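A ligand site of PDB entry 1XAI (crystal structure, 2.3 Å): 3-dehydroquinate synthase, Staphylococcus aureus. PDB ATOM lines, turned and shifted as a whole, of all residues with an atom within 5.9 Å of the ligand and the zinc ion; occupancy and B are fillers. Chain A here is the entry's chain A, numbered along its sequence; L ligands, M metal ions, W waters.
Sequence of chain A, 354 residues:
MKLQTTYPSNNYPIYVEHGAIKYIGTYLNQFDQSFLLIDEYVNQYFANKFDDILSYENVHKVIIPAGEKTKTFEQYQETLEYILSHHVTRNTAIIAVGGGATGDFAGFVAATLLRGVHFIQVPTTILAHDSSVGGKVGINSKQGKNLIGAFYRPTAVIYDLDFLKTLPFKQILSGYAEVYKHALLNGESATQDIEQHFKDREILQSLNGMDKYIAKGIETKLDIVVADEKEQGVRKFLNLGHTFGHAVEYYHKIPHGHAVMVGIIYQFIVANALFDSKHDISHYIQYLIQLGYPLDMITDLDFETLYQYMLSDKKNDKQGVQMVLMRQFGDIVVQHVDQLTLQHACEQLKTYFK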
ATOM      1  N   ASP A 130     -30.873  21.493  14.957  1.00  0.00           N
ATOM      2  CA  ASP A 130     -30.485  21.549  16.348  1.00  0.00           C
ATOM      3  C   ASP A 130     -29.852  22.906  16.682  1.00  0.00           C
ATOM      4  O   ASP A 130     -30.446  23.690  17.430  1.00  0.00           O
ATOM      5  CB  ASP A 130     -29.476  20.433  16.631  1.00  0.00           C
ATOM      6  CG  ASP A 130     -28.797  20.597  17.951  1.00  0.00           C
ATOM      7  OD1 ASP A 130     -29.492  20.853  18.949  1.00  0.00           O
ATOM      8  OD2 ASP A 130     -27.547  20.465  17.993  1.00  0.00           O
ATOM      9  N   SER A 131     -28.684  23.186  16.116  1.00  0.00           N
ATOM     10  CA  SER A 131     -27.982  24.436  16.369  1.00  0.00           C
ATOM     11  C   SER A 131     -28.752  25.754  16.146  1.00  0.00           C
ATOM     12  O   SER A 131     -28.429  26.769  16.768  1.00  0.00           O
ATOM     13  CB  SER A 131     -26.689  24.491  15.553  1.00  0.00           C
ATOM     14  OG  SER A 131     -26.939  24.503  14.161  1.00  0.00           O
ATOM     15  N   VAL A 133     -31.839  26.420  17.001  1.00  0.00           N
ATOM     16  CA  VAL A 133     -32.858  26.678  17.996  1.00  0.00           C
ATOM     17  C   VAL A 133     -32.231  26.685  19.405  1.00  0.00           C
ATOM     18  O   VAL A 133     -31.344  25.890  19.708  1.00  0.00           O
ATOM     19  CB  VAL A 133     -33.967  25.595  17.906  1.00  0.00           C
ATOM     20  CG1 VAL A 133     -35.216  26.037  18.665  1.00  0.00           C
ATOM     21  CG2 VAL A 133     -34.295  25.321  16.440  1.00  0.00           C
ATOM     22  N   GLY A 134     -32.685  27.605  20.247  1.00  0.00           N
ATOM     23  CA  GLY A 134     -32.166  27.669  21.599  1.00  0.00           C
ATOM     24  C   GLY A 134     -31.392  28.931  21.924  1.00  0.00           C
ATOM     25  O   GLY A 134     -31.232  29.290  23.094  1.00  0.00           O
ATOM     26  N   LYS A 136     -28.100  29.460  21.541  1.00  0.00           N
ATOM     27  CA  LYS A 136     -26.670  29.326  21.862  1.00  0.00           C
ATOM     28  C   LYS A 136     -25.769  29.653  20.659  1.00  0.00           C
ATOM     29  O   LYS A 136     -25.806  28.968  19.632  1.00  0.00           O
ATOM     30  CB  LYS A 136     -26.340  27.912  22.338  1.00  0.00           C
ATOM     31  CG  LYS A 136     -26.520  27.687  23.825  1.00  0.00           C
ATOM     32  CD  LYS A 136     -25.964  26.327  24.255  1.00  0.00           C
ATOM     33  CE  LYS A 136     -26.332  26.003  25.685  1.00  0.00           C
ATOM     34  NZ  LYS A 136     -25.887  24.646  26.114  1.00  0.00           N
ATOM     35  N   LYS A 145     -14.252  23.705  21.979  1.00  0.00           N
ATOM     36  CA  LYS A 145     -15.388  24.181  21.205  1.00  0.00           C
ATOM     37  C   LYS A 145     -16.353  25.000  22.051  1.00  0.00           C
ATOM     38  O   LYS A 145     -16.575  24.698  23.217  1.00  0.00           O
ATOM     39  CB  LYS A 145     -16.119  22.971  20.582  1.00  0.00           C
ATOM     40  CG  LYS A 145     -17.332  23.313  19.734  1.00  0.00           C
ATOM     41  CD  LYS A 145     -17.863  22.055  19.049  1.00  0.00           C
ATOM     42  CE  LYS A 145     -19.236  22.260  18.413  1.00  0.00           C
ATOM     43  NZ  LYS A 145     -19.256  23.110  17.203  1.00  0.00           N
ATOM     44  N   ASN A 146     -16.891  26.056  21.452  1.00  0.00           N
ATOM     45  CA  ASN A 146     -17.877  26.937  22.112  1.00  0.00           C
ATOM     46  C   ASN A 146     -17.536  27.447  23.511  1.00  0.00           C
ATOM     47  O   ASN A 146     -18.383  27.369  24.423  1.00  0.00           O
ATOM     48  CB  ASN A 146     -19.228  26.227  22.190  1.00  0.00           C
ATOM     49  CG  ASN A 146     -19.609  25.575  20.891  1.00  0.00           C
ATOM     50  OD1 ASN A 146     -19.074  25.926  19.828  1.00  0.00           O
ATOM     51  ND2 ASN A 146     -20.549  24.631  20.955  1.00  0.00           N
ATOM     52  N   GLU A 178     -27.918  14.171  15.717  1.00  0.00           N
ATOM     53  CA  GLU A 178     -28.715  15.047  16.591  1.00  0.00           C
ATOM     54  C   GLU A 178     -30.173  14.616  16.520  1.00  0.00           C
ATOM     55  O   GLU A 178     -30.873  14.665  17.539  1.00  0.00           O
ATOM     56  CB  GLU A 178     -28.605  16.513  16.170  1.00  0.00           C
ATOM     57  CG  GLU A 178     -27.215  17.137  16.247  1.00  0.00           C
ATOM     58  CD  GLU A 178     -26.686  17.265  17.644  1.00  0.00           C
ATOM     59  OE1 GLU A 178     -25.498  17.614  17.797  1.00  0.00           O
ATOM     60  OE2 GLU A 178     -27.451  17.027  18.598  1.00  0.00           O
ATOM     61  N   LYS A 181     -30.274  11.715  18.714  1.00  0.00           N
ATOM     62  CA  LYS A 181     -30.098  12.088  20.117  1.00  0.00           C
ATOM     63  C   LYS A 181     -31.407  12.537  20.750  1.00  0.00           C
ATOM     64  O   LYS A 181     -31.722  12.178  21.879  1.00  0.00           O
ATOM     65  CB  LYS A 181     -29.068  13.215  20.243  1.00  0.00           C
ATOM     66  CG  LYS A 181     -28.655  13.519  21.690  1.00  0.00           C
ATOM     67  CD  LYS A 181     -28.048  14.913  21.841  1.00  0.00           C
ATOM     68  CE  LYS A 181     -28.959  16.003  21.269  1.00  0.00           C
ATOM     69  NZ  LYS A 181     -28.399  17.385  21.386  1.00  0.00           N
ATOM     70  N   LYS A 221     -36.606  20.023  21.186  1.00  0.00           N
ATOM     71  CA  LYS A 221     -35.663  20.967  21.753  1.00  0.00           C
ATOM     72  C   LYS A 221     -36.383  22.211  22.232  1.00  0.00           C
ATOM     73  O   LYS A 221     -36.149  22.688  23.339  1.00  0.00           O
ATOM     74  CB  LYS A 221     -34.596  21.378  20.724  1.00  0.00           C
ATOM     75  CG  LYS A 221     -33.383  22.080  21.357  1.00  0.00           C
ATOM     76  CD  LYS A 221     -32.371  22.536  20.302  1.00  0.00           C
ATOM     77  CE  LYS A 221     -31.128  23.076  20.966  1.00  0.00           C
ATOM     78  NZ  LYS A 221     -30.137  23.584  20.002  1.00  0.00           N
ATOM     79  N   VAL A 225     -35.442  24.093  25.718  1.00  0.00           N
ATOM     80  CA  VAL A 225     -34.867  25.433  25.716  1.00  0.00           C
ATOM     81  C   VAL A 225     -35.825  26.471  26.285  1.00  0.00           C
ATOM     82  O   VAL A 225     -35.388  27.420  26.942  1.00  0.00           O
ATOM     83  CB  VAL A 225     -34.389  25.870  24.295  1.00  0.00           C
ATOM     84  CG1 VAL A 225     -33.419  24.847  23.737  1.00  0.00           C
ATOM     85  CG2 VAL A 225     -35.573  26.054  23.363  1.00  0.00           C
ATOM     86  N   GLU A 231     -29.792  26.876  30.505  1.00  0.00           N
ATOM     87  CA  GLU A 231     -29.220  25.573  30.858  1.00  0.00           C
ATOM     88  C   GLU A 231     -29.015  25.529  32.364  1.00  0.00           C
ATOM     89  O   GLU A 231     -27.903  25.298  32.848  1.00  0.00           O
ATOM     90  CB  GLU A 231     -27.878  25.321  30.147  1.00  0.00           C
ATOM     91  CG  GLU A 231     -27.388  23.852  30.199  1.00  0.00           C
ATOM     92  CD  GLU A 231     -25.936  23.639  29.738  1.00  0.00           C
ATOM     93  OE1 GLU A 231     -25.520  24.265  28.731  1.00  0.00           O
ATOM     94  OE2 GLU A 231     -25.205  22.842  30.372  1.00  0.00           O
ATOM     95  N   ARG A 235     -31.797  21.562  30.463  1.00  0.00           N
ATOM     96  CA  ARG A 235     -31.223  21.741  29.122  1.00  0.00           C
ATOM     97  C   ARG A 235     -29.865  21.054  29.025  1.00  0.00           C
ATOM     98  O   ARG A 235     -29.283  20.933  27.951  1.00  0.00           O
ATOM     99  CB  ARG A 235     -31.067  23.233  28.765  1.00  0.00           C
ATOM    100  CG  ARG A 235     -30.600  23.472  27.337  1.00  0.00           C
ATOM    101  CD  ARG A 235     -30.644  24.949  26.906  1.00  0.00           C
ATOM    102  NE  ARG A 235     -30.151  25.087  25.538  1.00  0.00           N
ATOM    103  CZ  ARG A 235     -30.269  26.160  24.752  1.00  0.00           C
ATOM    104  NH1 ARG A 235     -30.874  27.276  25.166  1.00  0.00           N
ATOM    105  NH2 ARG A 235     -29.792  26.105  23.515  1.00  0.00           N
ATOM    106  N   LEU A 238     -29.522  18.137  26.456  1.00  0.00           N
ATOM    107  CA  LEU A 238     -29.271  18.220  25.019  1.00  0.00           C
ATOM    108  C   LEU A 238     -27.787  17.926  24.800  1.00  0.00           C
ATOM    109  O   LEU A 238     -27.326  17.727  23.677  1.00  0.00           O
ATOM    110  CB  LEU A 238     -29.620  19.610  24.502  1.00  0.00           C
ATOM    111  CG  LEU A 238     -31.036  20.129  24.772  1.00  0.00           C
ATOM    112  CD1 LEU A 238     -31.273  21.409  23.983  1.00  0.00           C
ATOM    113  CD2 LEU A 238     -32.046  19.072  24.349  1.00  0.00           C
ATOM    114  N   ASN A 239     -27.041  17.884  25.911  1.00  0.00           N
ATOM    115  CA  ASN A 239     -25.614  17.605  25.932  1.00  0.00           C
ATOM    116  C   ASN A 239     -25.331  16.110  25.993  1.00  0.00           C
ATOM    117  O   ASN A 239     -24.202  15.690  26.281  1.00  0.00           O
ATOM    118  CB  ASN A 239     -24.977  18.286  27.148  1.00  0.00           C
ATOM    119  CG  ASN A 239     -24.146  19.496  26.783  1.00  0.00           C
ATOM    120  OD1 ASN A 239     -23.061  19.364  26.219  1.00  0.00           O
ATOM    121  ND2 ASN A 239     -24.659  20.688  27.100  1.00  0.00           N
ATOM    122  N   HIS A 242     -22.078  14.615  24.486  1.00  0.00           N
ATOM    123  CA  HIS A 242     -21.218  15.685  23.990  1.00  0.00           C
ATOM    124  C   HIS A 242     -19.971  15.873  24.842  1.00  0.00           C
ATOM    125  O   HIS A 242     -19.014  16.518  24.410  1.00  0.00           O
ATOM    126  CB  HIS A 242     -21.962  17.015  23.936  1.00  0.00           C
ATOM    127  CG  HIS A 242     -23.001  17.080  22.870  1.00  0.00           C
ATOM    128  ND1 HIS A 242     -24.008  16.151  22.744  1.00  0.00           N
ATOM    129  CD2 HIS A 242     -23.211  18.001  21.891  1.00  0.00           C
ATOM    130  CE1 HIS A 242     -24.793  16.488  21.742  1.00  0.00           C
ATOM    131  NE2 HIS A 242     -24.337  17.601  21.206  1.00  0.00           N
ATOM    132  N   HIS A 246     -17.435  16.248  22.276  1.00  0.00           N
ATOM    133  CA  HIS A 246     -16.761  17.511  22.013  1.00  0.00           C
ATOM    134  C   HIS A 246     -15.250  17.361  22.059  1.00  0.00           C
ATOM    135  O   HIS A 246     -14.526  18.087  21.376  1.00  0.00           O
ATOM    136  CB  HIS A 246     -17.205  18.573  23.004  1.00  0.00           C
ATOM    137  CG  HIS A 246     -18.437  19.310  22.595  1.00  0.00           C
ATOM    138  ND1 HIS A 246     -19.194  20.055  23.476  1.00  0.00           N
ATOM    139  CD2 HIS A 246     -19.029  19.443  21.387  1.00  0.00           C
ATOM    140  CE1 HIS A 246     -20.198  20.622  22.825  1.00  0.00           C
ATOM    141  NE2 HIS A 246     -20.121  20.265  21.558  1.00  0.00           N
ATOM    142  N   HIS A 256     -19.259  16.915  13.687  1.00  0.00           N
ATOM    143  CA  HIS A 256     -19.956  16.976  14.959  1.00  0.00           C
ATOM    144  C   HIS A 256     -20.808  15.755  15.278  1.00  0.00           C
ATOM    145  O   HIS A 256     -20.654  15.173  16.348  1.00  0.00           O
ATOM    146  CB  HIS A 256     -20.830  18.227  15.034  1.00  0.00           C
ATOM    147  CG  HIS A 256     -21.339  18.503  16.407  1.00  0.00           C
ATOM    148  ND1 HIS A 256     -20.529  18.465  17.523  1.00  0.00           N
ATOM    149  CD2 HIS A 256     -22.588  18.771  16.855  1.00  0.00           C
ATOM    150  CE1 HIS A 256     -21.258  18.705  18.595  1.00  0.00           C
ATOM    151  NE2 HIS A 256     -22.506  18.901  18.218  1.00  0.00           N
ATOM    152  N   VAL A 260     -20.533  12.916  18.146  1.00  0.00           N
ATOM    153  CA  VAL A 260     -21.666  12.739  19.059  1.00  0.00           C
ATOM    154  C   VAL A 260     -22.084  11.255  19.146  1.00  0.00           C
ATOM    155  O   VAL A 260     -22.271  10.734  20.248  1.00  0.00           O
ATOM    156  CB  VAL A 260     -22.886  13.626  18.656  1.00  0.00           C
ATOM    157  CG1 VAL A 260     -24.145  13.136  19.359  1.00  0.00           C
ATOM    158  CG2 VAL A 260     -22.636  15.070  19.052  1.00  0.00           C
ATOM    159  N   LYS A 314     -18.163  22.737  29.683  1.00  0.00           N
ATOM    160  CA  LYS A 314     -19.013  23.735  30.312  1.00  0.00           C
ATOM    161  C   LYS A 314     -20.009  23.202  31.330  1.00  0.00           C
ATOM    162  O   LYS A 314     -20.773  23.965  31.919  1.00  0.00           O
ATOM    163  CB  LYS A 314     -19.769  24.531  29.232  1.00  0.00           C
ATOM    164  CG  LYS A 314     -18.914  25.502  28.436  1.00  0.00           C
ATOM    165  CD  LYS A 314     -19.760  26.358  27.485  1.00  0.00           C
ATOM    166  CE  LYS A 314     -20.295  25.545  26.324  1.00  0.00           C
ATOM    167  NZ  LYS A 314     -19.185  25.021  25.465  1.00  0.00           N
HETATM  168  C1  LIG L   1     -28.058  23.131  23.371  1.00  0.00           C
HETATM  169  O1  LIG L   1     -28.367  23.193  24.615  1.00  0.00           O
HETATM  170  O2  LIG L   1     -28.568  23.833  22.468  1.00  0.00           O
HETATM  171  C2  LIG L   1     -26.956  22.110  23.037  1.00  0.00           C
HETATM  172  O3  LIG L   1     -26.688  21.294  24.177  1.00  0.00           O
HETATM  173  C3  LIG L   1     -27.293  21.179  21.854  1.00  0.00           C
HETATM  174  C4  LIG L   1     -26.061  20.440  21.311  1.00  0.00           C
HETATM  175  O4  LIG L   1     -26.370  19.749  20.076  1.00  0.00           O
HETATM  176  C5  LIG L   1     -24.860  21.440  21.060  1.00  0.00           C
HETATM  177  O5  LIG L   1     -23.750  20.718  20.625  1.00  0.00           O
HETATM  178  C6  LIG L   1     -24.563  22.196  22.374  1.00  0.00           C
HETATM  179  C7  LIG L   1     -23.353  23.115  22.364  1.00  0.00           C
HETATM  180  C8  LIG L   1     -25.730  23.011  22.732  1.00  0.00           C
HETATM  181  P1  LIG L   1     -22.453  23.316  23.935  1.00  0.00           P
HETATM  182  O6  LIG L   1     -22.322  21.982  24.579  1.00  0.00           O
HETATM  183  O7  LIG L   1     -23.350  24.280  24.692  1.00  0.00           O
HETATM  184  O8  LIG L   1     -21.081  23.934  23.467  1.00  0.00           O
HETATM  185 ZN    ZN M   1     -24.441  18.796  19.328  1.00  0.00          ZN
HETATM  186  O   HOH W   1     -29.035  26.549  20.563  1.00  0.00           O
HETATM  187  O   HOH W   2     -24.789  21.058  16.812  1.00  0.00           O
HETATM  188  O   HOH W   3     -22.540  22.838  27.742  1.00  0.00           O
HETATM  189  O   HOH W   4     -30.182  19.352  21.188  1.00  0.00           O
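The side-chain carboxylate (OE2) of Glu 178 is in salt-bridge range of the side-chain amino group (NZ) of Lys 181 (3.0 Å). The side-chain carboxylate (OD1) of Asp 130 is in salt-bridge range of the side-chain amino group (NZ) of Lys 221, at 3.0 Å. The backbone carbonyl oxygen (O) of Asn 146 sits at hydrogen-bond distance from the side-chain amino group (NZ) of Lys 314, 2.7 Å away. The guanidinium group of Arg 235 sits at hydrogen-bond distance from the backbone carbonyl oxygen of Gly 134 (2.9 Å). OE1 of Glu 231 lies within salt-bridge range of NZ of Lys 136 (2.7 Å). NZ of Lys 221 is in hydrogen-bond range of O of Val 133, 2.6 Å away. The side-chain amino group (NZ) of Lys 314 lies within hydrogen-bond range of the backbone carbonyl oxygen (O) of Lys 145. NZ of Lys 181 sits at hydrogen-bond distance from O of Leu 238 (2.6 Å).
Merely in contact with the zinc ion: Asp 130. Within 4 Å of the zinc ion: Asp 130, Glu 178, His 242 and His 256. The nearest printed residue that does not touch the zinc ion is Val 260 (4.1 Å).
Water W3 lies within hydrogen-bond range of ND2 of Asn 239 (3.1 Å), O6 of the ligand (3.3 Å) and OE1 of Glu 231 (3.4 Å). Water W4 bridges NZ of Lys 181 (2.7 Å) and OD1 of Asp 130 (2.8 Å).
The side-chain carboxylate of Asp 130 sits close to an oxygen (O4) of the ligand (2.5 Å). ND2 of Asn 146 sits at hydrogen-bond distance from O8 of the ligand (2.7 Å). O1 of the ligand lies within salt-bridge range of NE of Arg 235, at 2.8 Å. An oxygen (O7) of the ligand is in salt-bridge range of the side-chain amino group (NZ) of Lys 136. The side-chain amino group (NZ) of Lys 221 is in salt-bridge range of an oxygen (O2) of the ligand, at 2.9 Å. The side-chain amino group (NZ) of Lys 314 is in salt-bridge range of an oxygen (O8) of the ligand (3.0 Å). OD1 of Asn 239 sits close to O6 of the ligand (3.2 Å). NZ of Lys 181 lies close to O4 of the ligand.
Leu 238 touches the ligand. His 246 touches the ligand (CE1 to O6, 3.1 Å). Hydrophobic or aromatic side chains within 4 Å of the ligand: Leu 238, His 242, His 246 and His 256. Within 4 Å of the ligand: Asp 130, Lys 136, Asn 146, Glu 178, Lys 181, Lys 221, Arg 235, Leu 238, Asn 239, His 242, His 246, His 256 and Lys 314.
OE1 of Glu 178 is bound to the zinc ion, at 2.2 Å. NE2 of His 242 binds the zinc ion (2.2 Å). The zinc ion is bound by NE2 of His 256, at 2.2 Å. O4 of the ligand binds the zinc ion (2.3 Å). The zinc ion is bound by O5 of the ligand, at 2.4 Å.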
